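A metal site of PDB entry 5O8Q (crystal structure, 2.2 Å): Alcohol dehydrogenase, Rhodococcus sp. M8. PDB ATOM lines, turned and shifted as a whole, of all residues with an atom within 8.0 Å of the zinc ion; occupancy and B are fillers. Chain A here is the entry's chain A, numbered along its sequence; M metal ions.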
ATOM      1  N   TRP A  90      -2.854 -25.026 -23.934  1.00  0.00           N
ATOM      2  CA  TRP A  90      -1.496 -25.066 -23.370  1.00  0.00           C
ATOM      3  C   TRP A  90      -1.406 -24.327 -22.026  1.00  0.00           C
ATOM      4  O   TRP A  90      -1.817 -23.173 -21.914  1.00  0.00           O
ATOM      5  CB  TRP A  90      -0.466 -24.464 -24.347  1.00  0.00           C
ATOM      6  CG  TRP A  90      -0.279 -25.189 -25.654  1.00  0.00           C
ATOM      7  CD1 TRP A  90      -0.814 -26.399 -25.987  1.00  0.00           C
ATOM      8  CD2 TRP A  90       0.499 -24.770 -26.776  1.00  0.00           C
ATOM      9  NE1 TRP A  90      -0.435 -26.751 -27.268  1.00  0.00           N
ATOM     10  CE2 TRP A  90       0.377 -25.768 -27.772  1.00  0.00           C
ATOM     11  CE3 TRP A  90       1.284 -23.639 -27.039  1.00  0.00           C
ATOM     12  CZ2 TRP A  90       1.015 -25.660 -29.015  1.00  0.00           C
ATOM     13  CZ3 TRP A  90       1.931 -23.533 -28.287  1.00  0.00           C
ATOM     14  CH2 TRP A  90       1.780 -24.539 -29.261  1.00  0.00           C
ATOM     15  N   GLY A  91      -0.864 -25.020 -21.027  1.00  0.00           N
ATOM     16  CA  GLY A  91      -0.647 -24.471 -19.680  1.00  0.00           C
ATOM     17  C   GLY A  91       0.828 -24.303 -19.405  1.00  0.00           C
ATOM     18  O   GLY A  91       1.654 -24.578 -20.261  1.00  0.00           O
ATOM     19  N   CYS A  92       1.161 -23.863 -18.191  1.00  0.00           N
ATOM     20  CA  CYS A  92       2.552 -23.660 -17.783  1.00  0.00           C
ATOM     21  C   CYS A  92       3.309 -24.989 -17.571  1.00  0.00           C
ATOM     22  O   CYS A  92       4.524 -25.030 -17.644  1.00  0.00           O
ATOM     23  CB  CYS A  92       2.639 -22.806 -16.520  1.00  0.00           C
ATOM     24  SG  CYS A  92       2.133 -23.594 -14.977  1.00  0.00           S
ATOM     25  N   GLY A  93       2.575 -26.068 -17.277  1.00  0.00           N
ATOM     26  CA  GLY A  93       3.170 -27.376 -17.035  1.00  0.00           C
ATOM     27  C   GLY A  93       3.706 -27.606 -15.608  1.00  0.00           C
ATOM     28  O   GLY A  93       4.117 -28.735 -15.302  1.00  0.00           O
ATOM     29  N   ALA A  94       3.674 -26.577 -14.750  1.00  0.00           N
ATOM     30  CA  ALA A  94       4.329 -26.607 -13.424  1.00  0.00           C
ATOM     31  C   ALA A  94       3.414 -26.409 -12.205  1.00  0.00           C
ATOM     32  O   ALA A  94       3.804 -26.817 -11.121  1.00  0.00           O
ATOM     33  CB  ALA A  94       5.451 -25.570 -13.369  1.00  0.00           C
ATOM     34  N   CYS A  95       2.237 -25.791 -12.364  1.00  0.00           N
ATOM     35  CA  CYS A  95       1.339 -25.508 -11.233  1.00  0.00           C
ATOM     36  C   CYS A  95       0.559 -26.754 -10.797  1.00  0.00           C
ATOM     37  O   CYS A  95       0.599 -27.778 -11.466  1.00  0.00           O
ATOM     38  CB  CYS A  95       0.339 -24.387 -11.608  1.00  0.00           C
ATOM     39  SG  CYS A  95      -0.921 -24.812 -12.824  1.00  0.00           S
ATOM     40  N   HIS A  96      -0.169 -26.644  -9.687  1.00  0.00           N
ATOM     41  CA  HIS A  96      -0.927 -27.755  -9.137  1.00  0.00           C
ATOM     42  C   HIS A  96      -1.902 -28.346 -10.169  1.00  0.00           C
ATOM     43  O   HIS A  96      -1.978 -29.569 -10.318  1.00  0.00           O
ATOM     44  CB  HIS A  96      -1.663 -27.313  -7.871  1.00  0.00           C
ATOM     45  CG  HIS A  96      -2.286 -28.423  -7.085  1.00  0.00           C
ATOM     46  ND1 HIS A  96      -3.632 -28.703  -7.131  1.00  0.00           N
ATOM     47  CD2 HIS A  96      -1.752 -29.324  -6.217  1.00  0.00           C
ATOM     48  CE1 HIS A  96      -3.905 -29.704  -6.317  1.00  0.00           C
ATOM     49  NE2 HIS A  96      -2.783 -30.111  -5.757  1.00  0.00           N
ATOM     50  N   ALA A  97      -2.623 -27.481 -10.878  1.00  0.00           N
ATOM     51  CA  ALA A  97      -3.522 -27.922 -11.929  1.00  0.00           C
ATOM     52  C   ALA A  97      -2.776 -28.643 -13.069  1.00  0.00           C
ATOM     53  O   ALA A  97      -3.155 -29.748 -13.441  1.00  0.00           O
ATOM     54  CB  ALA A  97      -4.362 -26.760 -12.476  1.00  0.00           C
ATOM     55  N   CYS A  98      -1.712 -28.029 -13.587  1.00  0.00           N
ATOM     56  CA  CYS A  98      -0.937 -28.615 -14.682  1.00  0.00           C
ATOM     57  C   CYS A  98      -0.254 -29.936 -14.287  1.00  0.00           C
ATOM     58  O   CYS A  98      -0.112 -30.844 -15.113  1.00  0.00           O
ATOM     59  CB  CYS A  98       0.128 -27.626 -15.234  1.00  0.00           C
ATOM     60  SG  CYS A  98      -0.563 -26.259 -16.216  1.00  0.00           S
ATOM     61  N   ALA A  99       0.152 -30.055 -13.035  1.00  0.00           N
ATOM     62  CA  ALA A  99       0.760 -31.287 -12.532  1.00  0.00           C
ATOM     63  C   ALA A  99      -0.202 -32.489 -12.580  1.00  0.00           C
ATOM     64  O   ALA A  99       0.263 -33.624 -12.656  1.00  0.00           O
ATOM     65  CB  ALA A  99       1.308 -31.095 -11.122  1.00  0.00           C
ATOM     66  N   ARG A 102      -4.293 -30.972 -15.866  1.00  0.00           N
ATOM     67  CA  ARG A 102      -5.455 -30.109 -16.052  1.00  0.00           C
ATOM     68  C   ARG A 102      -5.003 -28.748 -16.537  1.00  0.00           C
ATOM     69  O   ARG A 102      -5.283 -27.730 -15.906  1.00  0.00           O
ATOM     70  CB  ARG A 102      -6.274 -29.986 -14.752  1.00  0.00           C
ATOM     71  CG  ARG A 102      -6.666 -31.314 -14.139  1.00  0.00           C
ATOM     72  CD  ARG A 102      -7.298 -31.163 -12.757  1.00  0.00           C
ATOM     73  NE  ARG A 102      -8.634 -30.574 -12.778  1.00  0.00           N
ATOM     74  CZ  ARG A 102      -9.749 -31.207 -13.111  1.00  0.00           C
ATOM     75  NH1 ARG A 102      -9.743 -32.481 -13.527  1.00  0.00           N
ATOM     76  NH2 ARG A 102     -10.906 -30.553 -13.014  1.00  0.00           N
ATOM     77  N   GLU A 103      -4.319 -28.720 -17.679  1.00  0.00           N
ATOM     78  CA  GLU A 103      -3.747 -27.484 -18.210  1.00  0.00           C
ATOM     79  C   GLU A 103      -4.833 -26.517 -18.701  1.00  0.00           C
ATOM     80  O   GLU A 103      -4.596 -25.303 -18.799  1.00  0.00           O
ATOM     81  CB  GLU A 103      -2.743 -27.774 -19.320  1.00  0.00           C
ATOM     82  CG  GLU A 103      -1.602 -28.676 -18.887  1.00  0.00           C
ATOM     83  CD  GLU A 103      -0.331 -28.558 -19.748  1.00  0.00           C
ATOM     84  OE1 GLU A 103      -0.252 -27.696 -20.651  1.00  0.00           O
ATOM     85  OE2 GLU A 103       0.617 -29.341 -19.485  1.00  0.00           O
ATOM     86  N   ASN A 104      -6.015 -27.052 -19.003  1.00  0.00           N
ATOM     87  CA  ASN A 104      -7.207 -26.226 -19.267  1.00  0.00           C
ATOM     88  C   ASN A 104      -7.574 -25.288 -18.116  1.00  0.00           C
ATOM     89  O   ASN A 104      -8.139 -24.223 -18.358  1.00  0.00           O
ATOM     90  CB  ASN A 104      -8.410 -27.096 -19.678  1.00  0.00           C
ATOM     91  CG  ASN A 104      -8.761 -28.173 -18.680  1.00  0.00           C
ATOM     92  OD1 ASN A 104      -7.877 -28.778 -18.067  1.00  0.00           O
ATOM     93  ND2 ASN A 104     -10.055 -28.450 -18.534  1.00  0.00           N
ATOM     94  N   TYR A 105      -7.209 -25.663 -16.893  1.00  0.00           N
ATOM     95  CA  TYR A 105      -7.435 -24.819 -15.702  1.00  0.00           C
ATOM     96  C   TYR A 105      -6.125 -24.285 -15.095  1.00  0.00           C
ATOM     97  O   TYR A 105      -6.066 -24.002 -13.899  1.00  0.00           O
ATOM     98  CB  TYR A 105      -8.246 -25.624 -14.678  1.00  0.00           C
ATOM     99  CG  TYR A 105      -9.609 -26.091 -15.190  1.00  0.00           C
ATOM    100  CD1 TYR A 105     -10.470 -25.211 -15.840  1.00  0.00           C
ATOM    101  CD2 TYR A 105     -10.034 -27.399 -15.004  1.00  0.00           C
ATOM    102  CE1 TYR A 105     -11.720 -25.618 -16.284  1.00  0.00           C
ATOM    103  CE2 TYR A 105     -11.285 -27.827 -15.461  1.00  0.00           C
ATOM    104  CZ  TYR A 105     -12.114 -26.922 -16.106  1.00  0.00           C
ATOM    105  OH  TYR A 105     -13.347 -27.307 -16.587  1.00  0.00           O
ATOM    106  N   CYS A 106      -5.110 -24.084 -15.935  1.00  0.00           N
ATOM    107  CA  CYS A 106      -3.839 -23.534 -15.472  1.00  0.00           C
ATOM    108  C   CYS A 106      -4.054 -22.138 -14.916  1.00  0.00           C
ATOM    109  O   CYS A 106      -4.676 -21.306 -15.571  1.00  0.00           O
ATOM    110  CB  CYS A 106      -2.826 -23.461 -16.613  1.00  0.00           C
ATOM    111  SG  CYS A 106      -1.256 -22.705 -16.111  1.00  0.00           S
ATOM    112  N   THR A 107      -3.527 -21.903 -13.716  1.00  0.00           N
ATOM    113  CA  THR A 107      -3.686 -20.615 -13.007  1.00  0.00           C
ATOM    114  C   THR A 107      -2.603 -19.566 -13.357  1.00  0.00           C
ATOM    115  O   THR A 107      -2.690 -18.470 -12.876  1.00  0.00           O
ATOM    116  CB  THR A 107      -3.684 -20.858 -11.468  1.00  0.00           C
ATOM    117  OG1 THR A 107      -2.597 -21.734 -11.112  1.00  0.00           O
ATOM    118  CG2 THR A 107      -5.007 -21.497 -11.019  1.00  0.00           C
ATOM    119  N   ARG A 108      -1.622 -19.929 -14.199  1.00  0.00           N
ATOM    120  CA  ARG A 108      -0.426 -19.125 -14.451  1.00  0.00           C
ATOM    121  C   ARG A 108      -0.138 -18.784 -15.933  1.00  0.00           C
ATOM    122  O   ARG A 108       0.780 -17.994 -16.223  1.00  0.00           O
ATOM    123  CB  ARG A 108       0.789 -19.849 -13.922  1.00  0.00           C
ATOM    124  CG  ARG A 108       0.875 -19.901 -12.392  1.00  0.00           C
ATOM    125  CD  ARG A 108       2.008 -20.714 -11.825  1.00  0.00           C
ATOM    126  NE  ARG A 108       3.288 -20.640 -12.533  1.00  0.00           N
ATOM    127  CZ  ARG A 108       4.327 -21.456 -12.329  1.00  0.00           C
ATOM    128  NH1 ARG A 108       5.443 -21.284 -13.054  1.00  0.00           N
ATOM    129  NH2 ARG A 108       4.294 -22.419 -11.391  1.00  0.00           N
ATOM    130  N   ALA A 109      -0.871 -19.386 -16.878  1.00  0.00           N
ATOM    131  CA  ALA A 109      -0.570 -19.245 -18.298  1.00  0.00           C
ATOM    132  C   ALA A 109      -0.694 -17.795 -18.812  1.00  0.00           C
ATOM    133  O   ALA A 109       0.119 -17.356 -19.626  1.00  0.00           O
ATOM    134  CB  ALA A 109      -1.465 -20.171 -19.119  1.00  0.00           C
ATOM    135  N   LEU A 112       2.393 -15.698 -17.782  1.00  0.00           N
ATOM    136  CA  LEU A 112       3.615 -16.150 -18.474  1.00  0.00           C
ATOM    137  C   LEU A 112       3.589 -15.914 -20.009  1.00  0.00           C
ATOM    138  O   LEU A 112       4.593 -16.175 -20.677  1.00  0.00           O
ATOM    139  CB  LEU A 112       3.893 -17.633 -18.174  1.00  0.00           C
ATOM    140  CG  LEU A 112       4.497 -17.945 -16.790  1.00  0.00           C
ATOM    141  CD1 LEU A 112       4.533 -19.430 -16.504  1.00  0.00           C
ATOM    142  CD2 LEU A 112       5.920 -17.368 -16.630  1.00  0.00           C
ATOM    143  N   ILE A 114       1.697 -17.574 -22.261  1.00  0.00           N
ATOM    144  CA  ILE A 114       1.496 -18.825 -22.977  1.00  0.00           C
ATOM    145  C   ILE A 114       0.084 -18.787 -23.533  1.00  0.00           C
ATOM    146  O   ILE A 114      -0.879 -18.702 -22.781  1.00  0.00           O
ATOM    147  CB  ILE A 114       1.717 -20.077 -22.062  1.00  0.00           C
ATOM    148  CG1 ILE A 114       3.197 -20.192 -21.669  1.00  0.00           C
ATOM    149  CG2 ILE A 114       1.281 -21.337 -22.766  1.00  0.00           C
ATOM    150  CD1 ILE A 114       3.477 -21.149 -20.538  1.00  0.00           C
ATOM    151  N   ARG A 135       4.845 -32.834 -24.428  1.00  0.00           N
ATOM    152  CA  ARG A 135       3.671 -33.179 -23.643  1.00  0.00           C
ATOM    153  C   ARG A 135       2.336 -32.708 -24.261  1.00  0.00           C
ATOM    154  O   ARG A 135       1.269 -33.125 -23.809  1.00  0.00           O
ATOM    155  CB  ARG A 135       3.798 -32.657 -22.187  1.00  0.00           C
ATOM    156  CG  ARG A 135       3.599 -31.164 -22.027  1.00  0.00           C
ATOM    157  CD  ARG A 135       3.721 -30.717 -20.575  1.00  0.00           C
ATOM    158  NE  ARG A 135       3.216 -29.369 -20.382  1.00  0.00           N
ATOM    159  CZ  ARG A 135       3.893 -28.248 -20.655  1.00  0.00           C
ATOM    160  NH1 ARG A 135       5.135 -28.265 -21.179  1.00  0.00           N
ATOM    161  NH2 ARG A 135       3.307 -27.066 -20.470  1.00  0.00           N
HETATM  162 ZN    ZN M   1      -0.087 -24.320 -15.008  1.00  0.00          ZN
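Gly 93 touches the zinc ion (N to ZN, 3.9 Å). Of the 21 residues printed, 5 come within 4 Å of the zinc ion.
SG of Cys 106 sits close to N of Arg 108 (3.4 Å). The side-chain sulfur of Cys 106 lies close to the backbone NH of Ala 109, at 3.4 Å. The side-chain sulfur (SG) of Cys 98 lies close to the backbone NH (N) of Gly 93, 3.3 Å away. The backbone NH (N) of Ala 94 sits close to the side-chain sulfur (SG) of Cys 92. The backbone NH (N) of Ala 97 lies close to the side-chain sulfur (SG) of Cys 95.
The zinc ion is bound by SG of Cys 106, at 2.3 Å. The side-chain sulfur (SG) of Cys 98 binds the zinc ion. The side-chain sulfur (SG) of Cys 92 is bound to the zinc ion (2.3 Å). SG of Cys 95 binds the zinc ion (2.4 Å).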
